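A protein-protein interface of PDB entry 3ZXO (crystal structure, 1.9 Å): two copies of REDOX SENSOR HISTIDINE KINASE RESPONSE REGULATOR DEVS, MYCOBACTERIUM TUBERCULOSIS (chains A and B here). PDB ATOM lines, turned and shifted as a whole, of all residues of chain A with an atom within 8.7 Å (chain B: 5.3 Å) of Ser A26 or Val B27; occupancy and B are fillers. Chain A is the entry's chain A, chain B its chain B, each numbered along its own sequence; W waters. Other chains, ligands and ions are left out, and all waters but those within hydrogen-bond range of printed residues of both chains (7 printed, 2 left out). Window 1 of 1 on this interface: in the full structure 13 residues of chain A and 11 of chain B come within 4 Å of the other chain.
The guanidinium group of Arg A24 lies within hydrogen-bond range of the side-chain hydroxyl of Thr B25 (2.8 Å).
The side-chain carboxylate of Asp B12 sits at hydrogen-bond distance from the side-chain hydroxyl of Ser A26, at 2.8 Å.
N of Thr A25 sits at hydrogen-bond distance from O of Thr B25 (3.1 Å).
The backbone carbonyl oxygen (O) of Thr A25 sits at hydrogen-bond distance from the backbone NH (N) of Val B27 (2.9 Å).
OE1 of Gln B28 lies close to OD2 of Asp A12 (3.5 Å).
O of Val A27 is in hydrogen-bond range of N of Phe B29, 2.8 Å away.
The backbone carbonyl oxygen (O) of Val B27 is in hydrogen-bond range of the backbone NH (N) of Val A27.
The backbone carbonyl oxygen (O) of Phe B29 lies within hydrogen-bond range of the backbone NH (N) of Phe A29 (2.9 Å).
The side-chain hydroxyl (OG1) of Thr A25 is in hydrogen-bond range of the side-chain hydroxyl (OG) of Ser B26 (3.4 Å).
The backbone NH (N) of Gln A28 sits at hydrogen-bond distance from the backbone carbonyl oxygen (O) of Val A66 (2.8 Å).
The backbone NH (N) of Arg A24 is in hydrogen-bond range of the backbone carbonyl oxygen (O) of Ser A62 (3.1 Å).
O of Gln A28 sits at hydrogen-bond distance from N of Val A68 (2.9 Å).
NE of Arg A67 lies within salt-bridge range of OE1 of Glu A77, at 3.6 Å.
The backbone carbonyl oxygen (O) of Val B66 sits at hydrogen-bond distance from the backbone NH (N) of Gln B28.
O of Ser A26 sits at hydrogen-bond distance from N of Val A66.
Among the printed residues, merely in contact across the chains: Ser A26 with Val B27 (3.3 Å), Ser A26 with Phe B29 (3.5 Å), Val A27 with Gln B28 (3.1 Å), Gln A28 with Arg B8 (3.9 Å), Gln A28 with Phe B29 (3.6 Å) and Arg A67 with Arg B8 (3.7 Å).
Printed residues of chain B within 4 Å of Asp A12: Gln B28 (3.5 Å).
Printed residues of chain B within 4 Å of Arg A24: Thr B25 (2.8 Å).
Of chain B, only Asp B12, Val B27 and Phe B29 come within 4 Å of Ser A26.
Printed residues of chain B within 4 Å of Val A27: Val B27 (2.8 Å), Gln B28 (3.1 Å) and Phe B29 (2.8 Å).
Printed residues of chain B within 4 Å of Gln A28: Arg B8 (3.9 Å) and Phe B29 (3.6 Å).
Thr A63 touches none of the printed residues of chain B.
Printed residues of chain B within 4 Å of Arg A67: Arg B8.
The nearest residue of chain A that does not touch Val B27 is Gln A28 (5.5 Å).
Hydrophobic or aromatic side chains of chain A within 4 Å of the printed part of chain B: Phe A29.
Along chain A the printed residues that touch a printed residue of chain B span positions 12 to 67.
Printed residues of chain B that touch a printed residue of chain A: Arg B8, Asp B12, Thr B25, Ser B26, Val B27, Gln B28 and Phe B29.
Hydrophobic or aromatic side chains of chain B that line the printed part of chain A: Phe B29.
Among the printed residues, no Asp or Glu carboxylate lies within 4 Å of a Lys or Arg side-chain nitrogen of the other chain.
Asp A12 touches Gln B28, but with the chains exchanged Gln A28 does not touch Asp B12 (7.2 Å).
Thr A25 touches Ser B26, but with the chains exchanged Ser A26 does not touch Thr B25 (5.8 Å).
Thr A25 touches Val B27, but with the chains exchanged Val A27 does not touch Thr B25 (8.4 Å).
Ser A26 touches Val B27, but with the chains exchanged Val A27 does not touch Ser B26 (5.8 Å).
Of the 15 pairs that touch across the chains among the printed residues, 3 have their exchanged pair printed and touching as well.
Water W6 lies within hydrogen-bond range of OG of Ser B26 (2.6 Å), O of Val B27 (2.8 Å) and OG1 of Thr A25 (2.9 Å).
Water W7 bridges the guanidinium group (NE) of Arg B8 (2.7 Å) and the side-chain amide oxygen (OE1) of Gln A28 (3.5 Å).
Water W2 lies within hydrogen-bond range of OD2 of Asp B12 (2.8 Å), NH1 of Arg B8 (2.8 Å) and OG1 of Thr A65 (2.9 Å).
Water W4 bridges the side-chain hydroxyl of Thr B25 (2.8 Å) and the backbone carbonyl oxygen of Thr A25 (3.1 Å).
Water W1 bridges O of Leu A23 (2.9 Å) and N of Thr B25 (2.9 Å).
Water W3 lies within hydrogen-bond range of OD2 of Asp A12 (3.0 Å) and OE1 of Gln B28 (3.2 Å).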
ATOM      1  N   ILE A  11      10.099   0.542  -0.882  1.00  0.00           N
ATOM      2  CA  ILE A  11       9.464   1.501   0.032  1.00  0.00           C
ATOM      3  C   ILE A  11      10.027   2.902  -0.197  1.00  0.00           C
ATOM      4  O   ILE A  11       9.260   3.858  -0.316  1.00  0.00           O
ATOM      5  CB  ILE A  11       9.577   1.095   1.497  1.00  0.00           C
ATOM      6  CG1 ILE A  11       8.627  -0.078   1.774  1.00  0.00           C
ATOM      7  CG2 ILE A  11       9.324   2.333   2.467  1.00  0.00           C
ATOM      8  CD1 ILE A  11       8.787  -0.711   3.147  1.00  0.00           C
ATOM      9  N   ASP A  12      11.347   3.026  -0.308  1.00  0.00           N
ATOM     10  CA  ASP A  12      11.901   4.354  -0.620  1.00  0.00           C
ATOM     11  C   ASP A  12      11.355   4.896  -1.928  1.00  0.00           C
ATOM     12  O   ASP A  12      11.065   6.103  -2.021  1.00  0.00           O
ATOM     13  CB  ASP A  12      13.418   4.336  -0.711  1.00  0.00           C
ATOM     14  CG  ASP A  12      14.060   4.394   0.629  1.00  0.00           C
ATOM     15  OD1 ASP A  12      13.429   4.914   1.583  1.00  0.00           O
ATOM     16  OD2 ASP A  12      15.199   3.900   0.727  1.00  0.00           O
ATOM     17  N   VAL A  15       7.661   6.134  -1.604  1.00  0.00           N
ATOM     18  CA  VAL A  15       7.704   7.483  -0.994  1.00  0.00           C
ATOM     19  C   VAL A  15       8.104   8.582  -2.012  1.00  0.00           C
ATOM     20  O   VAL A  15       7.410   9.603  -2.093  1.00  0.00           O
ATOM     21  CB  VAL A  15       8.589   7.506   0.282  1.00  0.00           C
ATOM     22  CG1 VAL A  15       8.722   8.951   0.872  1.00  0.00           C
ATOM     23  CG2 VAL A  15       8.016   6.528   1.348  1.00  0.00           C
ATOM     24  N   ALA A  19       4.690  10.828  -2.704  1.00  0.00           N
ATOM     25  CA  ALA A  19       4.536  11.974  -1.751  1.00  0.00           C
ATOM     26  C   ALA A  19       4.370  13.281  -2.540  1.00  0.00           C
ATOM     27  O   ALA A  19       5.144  13.562  -3.449  1.00  0.00           O
ATOM     28  CB  ALA A  19       5.741  12.076  -0.840  1.00  0.00           C
ATOM     29  N   LEU A  23       5.514  18.251   0.391  1.00  0.00           N
ATOM     30  CA  LEU A  23       5.757  17.698   1.736  1.00  0.00           C
ATOM     31  C   LEU A  23       7.206  17.324   1.924  1.00  0.00           C
ATOM     32  O   LEU A  23       7.847  16.933   0.964  1.00  0.00           O
ATOM     33  CB  LEU A  23       4.888  16.442   1.965  1.00  0.00           C
ATOM     34  CG  LEU A  23       3.402  16.666   1.667  1.00  0.00           C
ATOM     35  CD1 LEU A  23       2.587  15.360   1.792  1.00  0.00           C
ATOM     36  CD2 LEU A  23       2.788  17.825   2.554  1.00  0.00           C
ATOM     37  N   ARG A  24       7.718  17.421   3.146  1.00  0.00           N
ATOM     38  CA  ARG A  24       9.037  16.841   3.436  1.00  0.00           C
ATOM     39  C   ARG A  24       8.776  15.396   3.791  1.00  0.00           C
ATOM     40  O   ARG A  24       7.722  15.101   4.361  1.00  0.00           O
ATOM     41  CB  ARG A  24       9.644  17.492   4.672  1.00  0.00           C
ATOM     42  CG  ARG A  24       9.987  18.943   4.446  1.00  0.00           C
ATOM     43  CD  ARG A  24      10.986  19.449   5.490  1.00  0.00           C
ATOM     44  NE  ARG A  24      11.076  20.923   5.359  1.00  0.00           N
ATOM     45  CZ  ARG A  24      11.798  21.559   4.432  1.00  0.00           C
ATOM     46  NH1 ARG A  24      12.534  20.889   3.555  1.00  0.00           N
ATOM     47  NH2 ARG A  24      11.805  22.882   4.397  1.00  0.00           N
ATOM     48  N   THR A  25       9.704  14.493   3.501  1.00  0.00           N
ATOM     49  CA  THR A  25       9.499  13.118   4.006  1.00  0.00           C
ATOM     50  C   THR A  25      10.721  12.646   4.726  1.00  0.00           C
ATOM     51  O   THR A  25      11.845  13.091   4.428  1.00  0.00           O
ATOM     52  CB  THR A  25       9.198  12.095   2.862  1.00  0.00           C
ATOM     53  OG1 THR A  25      10.336  12.004   1.986  1.00  0.00           O
ATOM     54  CG2 THR A  25       7.910  12.514   2.058  1.00  0.00           C
ATOM     55  N   SER A  26      10.504  11.695   5.626  1.00  0.00           N
ATOM     56  CA  SER A  26      11.567  11.065   6.393  1.00  0.00           C
ATOM     57  C   SER A  26      11.183   9.597   6.545  1.00  0.00           C
ATOM     58  O   SER A  26      10.079   9.306   7.009  1.00  0.00           O
ATOM     59  CB  SER A  26      11.710  11.732   7.765  1.00  0.00           C
ATOM     60  OG  SER A  26      12.656  11.014   8.565  1.00  0.00           O
ATOM     61  N   VAL A  27      12.069   8.682   6.150  1.00  0.00           N
ATOM     62  CA  VAL A  27      11.778   7.261   6.235  1.00  0.00           C
ATOM     63  C   VAL A  27      12.912   6.574   7.007  1.00  0.00           C
ATOM     64  O   VAL A  27      14.093   6.741   6.659  1.00  0.00           O
ATOM     65  CB  VAL A  27      11.635   6.658   4.855  1.00  0.00           C
ATOM     66  CG1 VAL A  27      11.238   5.173   4.944  1.00  0.00           C
ATOM     67  CG2 VAL A  27      10.567   7.466   4.062  1.00  0.00           C
ATOM     68  N   GLN A  28      12.533   5.852   8.065  1.00  0.00           N
ATOM     69  CA  GLN A  28      13.459   5.062   8.843  1.00  0.00           C
ATOM     70  C   GLN A  28      13.127   3.576   8.769  1.00  0.00           C
ATOM     71  O   GLN A  28      11.983   3.174   8.995  1.00  0.00           O
ATOM     72  CB  GLN A  28      13.439   5.520  10.287  1.00  0.00           C
ATOM     73  CG  GLN A  28      14.376   4.681  11.143  1.00  0.00           C
ATOM     74  CD  GLN A  28      14.500   5.210  12.508  1.00  0.00           C
ATOM     75  OE1 GLN A  28      13.517   5.623  13.114  1.00  0.00           O
ATOM     76  NE2 GLN A  28      15.714   5.189  13.033  1.00  0.00           N
ATOM     77  N   PHE A  29      14.146   2.773   8.464  1.00  0.00           N
ATOM     78  CA  PHE A  29      14.038   1.339   8.476  1.00  0.00           C
ATOM     79  C   PHE A  29      14.694   0.782   9.749  1.00  0.00           C
ATOM     80  O   PHE A  29      15.776   1.232  10.135  1.00  0.00           O
ATOM     81  CB  PHE A  29      14.706   0.778   7.241  1.00  0.00           C
ATOM     82  CG  PHE A  29      14.086   1.260   5.963  1.00  0.00           C
ATOM     83  CD1 PHE A  29      12.916   0.698   5.509  1.00  0.00           C
ATOM     84  CD2 PHE A  29      14.643   2.324   5.255  1.00  0.00           C
ATOM     85  CE1 PHE A  29      12.325   1.126   4.320  1.00  0.00           C
ATOM     86  CE2 PHE A  29      14.052   2.782   4.072  1.00  0.00           C
ATOM     87  CZ  PHE A  29      12.904   2.169   3.600  1.00  0.00           C
ATOM     88  N   VAL A  52       1.110   7.332   1.904  1.00  0.00           N
ATOM     89  CA  VAL A  52       1.841   8.479   1.406  1.00  0.00           C
ATOM     90  C   VAL A  52       1.065   9.206   0.297  1.00  0.00           C
ATOM     91  O   VAL A  52       1.043  10.446   0.235  1.00  0.00           O
ATOM     92  CB  VAL A  52       3.239   8.060   0.928  1.00  0.00           C
ATOM     93  CG1 VAL A  52       3.895   9.143   0.112  1.00  0.00           C
ATOM     94  CG2 VAL A  52       4.088   7.738   2.144  1.00  0.00           C
ATOM     95  N   SER A  62       5.006  20.801   6.437  1.00  0.00           N
ATOM     96  CA  SER A  62       4.720  19.576   7.198  1.00  0.00           C
ATOM     97  C   SER A  62       5.590  18.443   6.704  1.00  0.00           C
ATOM     98  O   SER A  62       6.121  18.495   5.575  1.00  0.00           O
ATOM     99  CB  SER A  62       3.221  19.213   7.110  1.00  0.00           C
ATOM    100  OG  SER A  62       2.828  18.835   5.800  1.00  0.00           O
ATOM    101  N   THR A  63       5.756  17.427   7.553  1.00  0.00           N
ATOM    102  CA  THR A  63       6.589  16.290   7.236  1.00  0.00           C
ATOM    103  C   THR A  63       5.753  15.038   7.404  1.00  0.00           C
ATOM    104  O   THR A  63       4.947  14.955   8.349  1.00  0.00           O
ATOM    105  CB  THR A  63       7.820  16.224   8.192  1.00  0.00           C
ATOM    106  OG1 THR A  63       8.599  17.396   8.007  1.00  0.00           O
ATOM    107  CG2 THR A  63       8.712  15.026   7.896  1.00  0.00           C
ATOM    108  N   LEU A  64       5.936  14.074   6.501  1.00  0.00           N
ATOM    109  CA  LEU A  64       5.476  12.714   6.758  1.00  0.00           C
ATOM    110  C   LEU A  64       6.672  11.921   7.176  1.00  0.00           C
ATOM    111  O   LEU A  64       7.654  11.832   6.419  1.00  0.00           O
ATOM    112  CB  LEU A  64       4.961  12.028   5.489  1.00  0.00           C
ATOM    113  CG  LEU A  64       3.644  12.410   4.876  1.00  0.00           C
ATOM    114  CD1 LEU A  64       3.540  11.595   3.537  1.00  0.00           C
ATOM    115  CD2 LEU A  64       2.501  12.084   5.834  1.00  0.00           C
ATOM    116  N   THR A  65       6.572  11.304   8.346  1.00  0.00           N
ATOM    117  CA  THR A  65       7.638  10.497   8.879  1.00  0.00           C
ATOM    118  C   THR A  65       7.156   9.057   8.760  1.00  0.00           C
ATOM    119  O   THR A  65       6.090   8.741   9.282  1.00  0.00           O
ATOM    120  CB  THR A  65       7.896  10.910  10.325  1.00  0.00           C
ATOM    121  OG1 THR A  65       8.283  12.291  10.321  1.00  0.00           O
ATOM    122  CG2 THR A  65       9.028  10.095  10.960  1.00  0.00           C
ATOM    123  N   VAL A  66       7.881   8.223   8.028  1.00  0.00           N
ATOM    124  CA  VAL A  66       7.524   6.802   7.904  1.00  0.00           C
ATOM    125  C   VAL A  66       8.577   5.948   8.630  1.00  0.00           C
ATOM    126  O   VAL A  66       9.798   6.114   8.396  1.00  0.00           O
ATOM    127  CB  VAL A  66       7.489   6.400   6.438  1.00  0.00           C
ATOM    128  CG1 VAL A  66       7.064   4.957   6.284  1.00  0.00           C
ATOM    129  CG2 VAL A  66       6.526   7.341   5.623  1.00  0.00           C
ATOM    130  N   ARG A  67       8.111   5.023   9.484  1.00  0.00           N
ATOM    131  CA  ARG A  67       9.005   4.077  10.146  1.00  0.00           C
ATOM    132  C   ARG A  67       8.549   2.651   9.841  1.00  0.00           C
ATOM    133  O   ARG A  67       7.391   2.278  10.090  1.00  0.00           O
ATOM    134  CB  ARG A  67       9.049   4.355  11.644  1.00  0.00           C
ATOM    135  CG  ARG A  67       9.146   5.831  11.922  1.00  0.00           C
ATOM    136  CD  ARG A  67       9.268   6.179  13.375  1.00  0.00           C
ATOM    137  NE  ARG A  67       8.735   7.517  13.580  1.00  0.00           N
ATOM    138  CZ  ARG A  67       8.943   8.248  14.662  1.00  0.00           C
ATOM    139  NH1 ARG A  67       9.700   7.770  15.646  1.00  0.00           N
ATOM    140  NH2 ARG A  67       8.393   9.446  14.752  1.00  0.00           N
ATOM    141  N   VAL A  68       9.442   1.874   9.233  1.00  0.00           N
ATOM    142  CA  VAL A  68       9.150   0.491   8.890  1.00  0.00           C
ATOM    143  C   VAL A  68      10.019  -0.383   9.791  1.00  0.00           C
ATOM    144  O   VAL A  68      11.255  -0.406   9.631  1.00  0.00           O
ATOM    145  CB  VAL A  68       9.423   0.210   7.405  1.00  0.00           C
ATOM    146  CG1 VAL A  68       9.182  -1.269   7.056  1.00  0.00           C
ATOM    147  CG2 VAL A  68       8.516   1.133   6.548  1.00  0.00           C
ATOM    148  N   GLU A  77       4.574   2.621  10.500  1.00  0.00           N
ATOM    149  CA  GLU A  77       3.944   3.749  11.193  1.00  0.00           C
ATOM    150  C   GLU A  77       4.192   5.046  10.430  1.00  0.00           C
ATOM    151  O   GLU A  77       5.350   5.356  10.141  1.00  0.00           O
ATOM    152  CB  GLU A  77       4.515   3.877  12.586  1.00  0.00           C
ATOM    153  CG  GLU A  77       4.000   5.081  13.324  1.00  0.00           C
ATOM    154  CD  GLU A  77       4.720   5.300  14.653  1.00  0.00           C
ATOM    155  OE1 GLU A  77       5.925   5.632  14.665  1.00  0.00           O
ATOM    156  OE2 GLU A  77       4.049   5.159  15.683  1.00  0.00           O
ATOM    157  N   VAL A  78       3.130   5.783  10.113  1.00  0.00           N
ATOM    158  CA  VAL A  78       3.264   7.006   9.335  1.00  0.00           C
ATOM    159  C   VAL A  78       2.752   8.137  10.210  1.00  0.00           C
ATOM    160  O   VAL A  78       1.608   8.092  10.667  1.00  0.00           O
ATOM    161  CB  VAL A  78       2.470   6.955   7.985  1.00  0.00           C
ATOM    162  CG1 VAL A  78       2.561   8.312   7.249  1.00  0.00           C
ATOM    163  CG2 VAL A  78       2.988   5.806   7.078  1.00  0.00           C
ATOM    164  N   THR A  79       3.596   9.133  10.457  1.00  0.00           N
ATOM    165  CA  THR A  79       3.208  10.273  11.300  1.00  0.00           C
ATOM    166  C   THR A  79       3.181  11.531  10.440  1.00  0.00           C
ATOM    167  O   THR A  79       4.142  11.813   9.698  1.00  0.00           O
ATOM    168  CB  THR A  79       4.175  10.437  12.488  1.00  0.00           C
ATOM    169  OG1 THR A  79       4.119   9.249  13.281  1.00  0.00           O
ATOM    170  CG2 THR A  79       3.755  11.542  13.384  1.00  0.00           C
ATOM    171  N   ARG B   8      18.578  10.732  14.762  1.00  0.00           N
ATOM    172  CA  ARG B   8      17.535  10.722  13.737  1.00  0.00           C
ATOM    173  C   ARG B   8      16.857  12.087  13.687  1.00  0.00           C
ATOM    174  O   ARG B   8      16.765  12.724  12.624  1.00  0.00           O
ATOM    175  CB  ARG B   8      16.521   9.594  14.014  1.00  0.00           C
ATOM    176  CG  ARG B   8      15.702   9.117  12.808  1.00  0.00           C
ATOM    177  CD  ARG B   8      14.522  10.062  12.464  1.00  0.00           C
ATOM    178  NE  ARG B   8      13.525  10.139  13.533  1.00  0.00           N
ATOM    179  CZ  ARG B   8      12.591  11.086  13.637  1.00  0.00           C
ATOM    180  NH1 ARG B   8      12.524  12.062  12.739  1.00  0.00           N
ATOM    181  NH2 ARG B   8      11.728  11.060  14.649  1.00  0.00           N
ATOM    182  N   ILE B  11      19.141  15.064  12.473  1.00  0.00           N
ATOM    183  CA  ILE B  11      19.346  15.026  11.002  1.00  0.00           C
ATOM    184  C   ILE B  11      18.091  15.556  10.284  1.00  0.00           C
ATOM    185  O   ILE B  11      18.185  16.362   9.382  1.00  0.00           O
ATOM    186  CB  ILE B  11      19.759  13.607  10.494  1.00  0.00           C
ATOM    187  CG1 ILE B  11      21.103  13.169  11.089  1.00  0.00           C
ATOM    188  CG2 ILE B  11      19.799  13.526   8.953  1.00  0.00           C
ATOM    189  CD1 ILE B  11      22.220  14.220  10.968  1.00  0.00           C
ATOM    190  N   ASP B  12      16.907  15.094  10.693  1.00  0.00           N
ATOM    191  CA  ASP B  12      15.652  15.624  10.131  1.00  0.00           C
ATOM    192  C   ASP B  12      15.533  17.118  10.275  1.00  0.00           C
ATOM    193  O   ASP B  12      15.114  17.796   9.335  1.00  0.00           O
ATOM    194  CB  ASP B  12      14.420  14.927  10.740  1.00  0.00           C
ATOM    195  CG  ASP B  12      14.051  13.663  10.006  1.00  0.00           C
ATOM    196  OD1 ASP B  12      14.341  13.569   8.801  1.00  0.00           O
ATOM    197  OD2 ASP B  12      13.449  12.761  10.630  1.00  0.00           O
ATOM    198  N   VAL B  15      18.026  19.102   7.954  1.00  0.00           N
ATOM    199  CA  VAL B  15      17.477  19.184   6.590  1.00  0.00           C
ATOM    200  C   VAL B  15      16.357  20.224   6.507  1.00  0.00           C
ATOM    201  O   VAL B  15      16.373  21.113   5.634  1.00  0.00           O
ATOM    202  CB  VAL B  15      17.011  17.771   6.136  1.00  0.00           C
ATOM    203  CG1 VAL B  15      16.325  17.827   4.745  1.00  0.00           C
ATOM    204  CG2 VAL B  15      18.212  16.804   6.116  1.00  0.00           C
ATOM    205  N   THR B  25      12.622  17.957   0.025  1.00  0.00           N
ATOM    206  CA  THR B  25      13.599  17.156   0.777  1.00  0.00           C
ATOM    207  C   THR B  25      13.042  15.805   1.201  1.00  0.00           C
ATOM    208  O   THR B  25      11.846  15.668   1.550  1.00  0.00           O
ATOM    209  CB  THR B  25      14.147  17.904   2.033  1.00  0.00           C
ATOM    210  OG1 THR B  25      13.076  18.199   2.942  1.00  0.00           O
ATOM    211  CG2 THR B  25      14.827  19.206   1.636  1.00  0.00           C
ATOM    212  N   SER B  26      13.946  14.825   1.224  1.00  0.00           N
ATOM    213  CA  SER B  26      13.634  13.455   1.595  1.00  0.00           C
ATOM    214  C   SER B  26      14.803  12.941   2.414  1.00  0.00           C
ATOM    215  O   SER B  26      15.931  13.006   1.941  1.00  0.00           O
ATOM    216  CB  SER B  26      13.542  12.605   0.332  1.00  0.00           C
ATOM    217  OG  SER B  26      13.411  11.225   0.631  1.00  0.00           O
ATOM    218  N   VAL B  27      14.539  12.427   3.614  1.00  0.00           N
ATOM    219  CA  VAL B  27      15.593  11.853   4.443  1.00  0.00           C
ATOM    220  C   VAL B  27      15.312  10.367   4.620  1.00  0.00           C
ATOM    221  O   VAL B  27      14.152   9.966   4.724  1.00  0.00           O
ATOM    222  CB  VAL B  27      15.692  12.551   5.808  1.00  0.00           C
ATOM    223  CG1 VAL B  27      16.949  12.039   6.590  1.00  0.00           C
ATOM    224  CG2 VAL B  27      15.802  14.031   5.618  1.00  0.00           C
ATOM    225  N   GLN B  28      16.364   9.559   4.602  1.00  0.00           N
ATOM    226  CA  GLN B  28      16.231   8.118   4.806  1.00  0.00           C
ATOM    227  C   GLN B  28      17.264   7.632   5.834  1.00  0.00           C
ATOM    228  O   GLN B  28      18.404   8.132   5.861  1.00  0.00           O
ATOM    229  CB  GLN B  28      16.453   7.392   3.493  1.00  0.00           C
ATOM    230  CG  GLN B  28      15.558   7.903   2.329  1.00  0.00           C
ATOM    231  CD  GLN B  28      15.988   7.402   0.973  1.00  0.00           C
ATOM    232  OE1 GLN B  28      17.065   6.829   0.824  1.00  0.00           O
ATOM    233  NE2 GLN B  28      15.160   7.637  -0.032  1.00  0.00           N
ATOM    234  N   PHE B  29      16.866   6.670   6.673  1.00  0.00           N
ATOM    235  CA  PHE B  29      17.724   6.144   7.742  1.00  0.00           C
ATOM    236  C   PHE B  29      17.698   4.624   7.672  1.00  0.00           C
ATOM    237  O   PHE B  29      16.635   4.030   7.540  1.00  0.00           O
ATOM    238  CB  PHE B  29      17.216   6.570   9.133  1.00  0.00           C
ATOM    239  CG  PHE B  29      17.177   8.049   9.357  1.00  0.00           C
ATOM    240  CD1 PHE B  29      18.317   8.720   9.810  1.00  0.00           C
ATOM    241  CD2 PHE B  29      15.998   8.782   9.142  1.00  0.00           C
ATOM    242  CE1 PHE B  29      18.302  10.109  10.034  1.00  0.00           C
ATOM    243  CE2 PHE B  29      15.953  10.163   9.383  1.00  0.00           C
ATOM    244  CZ  PHE B  29      17.130  10.843   9.847  1.00  0.00           C
ATOM    245  N   VAL B  66      18.685  12.801   1.443  1.00  0.00           N
ATOM    246  CA  VAL B  66      19.772  12.581   2.380  1.00  0.00           C
ATOM    247  C   VAL B  66      19.592  11.173   2.977  1.00  0.00           C
ATOM    248  O   VAL B  66      18.565  10.892   3.611  1.00  0.00           O
ATOM    249  CB  VAL B  66      19.735  13.606   3.495  1.00  0.00           C
ATOM    250  CG1 VAL B  66      20.923  13.392   4.480  1.00  0.00           C
ATOM    251  CG2 VAL B  66      19.734  15.032   2.921  1.00  0.00           C
ATOM    252  N   VAL B  68      21.135   8.259   5.450  1.00  0.00           N
ATOM    253  CA  VAL B  68      22.069   8.071   6.560  1.00  0.00           C
ATOM    254  C   VAL B  68      22.060   6.567   6.831  1.00  0.00           C
ATOM    255  O   VAL B  68      21.007   5.991   7.113  1.00  0.00           O
ATOM    256  CB  VAL B  68      21.620   8.843   7.801  1.00  0.00           C
ATOM    257  CG1 VAL B  68      22.538   8.559   8.999  1.00  0.00           C
ATOM    258  CG2 VAL B  68      21.588  10.335   7.530  1.00  0.00           C
HETATM  259  O   HOH W   1       9.985  18.830   0.742  1.00  0.00           O
HETATM  260  O   HOH W   2      10.825  13.506  11.077  1.00  0.00           O
HETATM  261  O   HOH W   3      17.444   4.263   2.696  1.00  0.00           O
HETATM  262  O   HOH W   4      12.945  15.941   4.655  1.00  0.00           O
HETATM  263  O   HOH W   5      10.034  14.472  -0.200  1.00  0.00           O
HETATM  264  O   HOH W   6      12.322  10.043   2.627  1.00  0.00           O
HETATM  265  O   HOH W   7      13.461   8.188  15.452  1.00  0.00           O
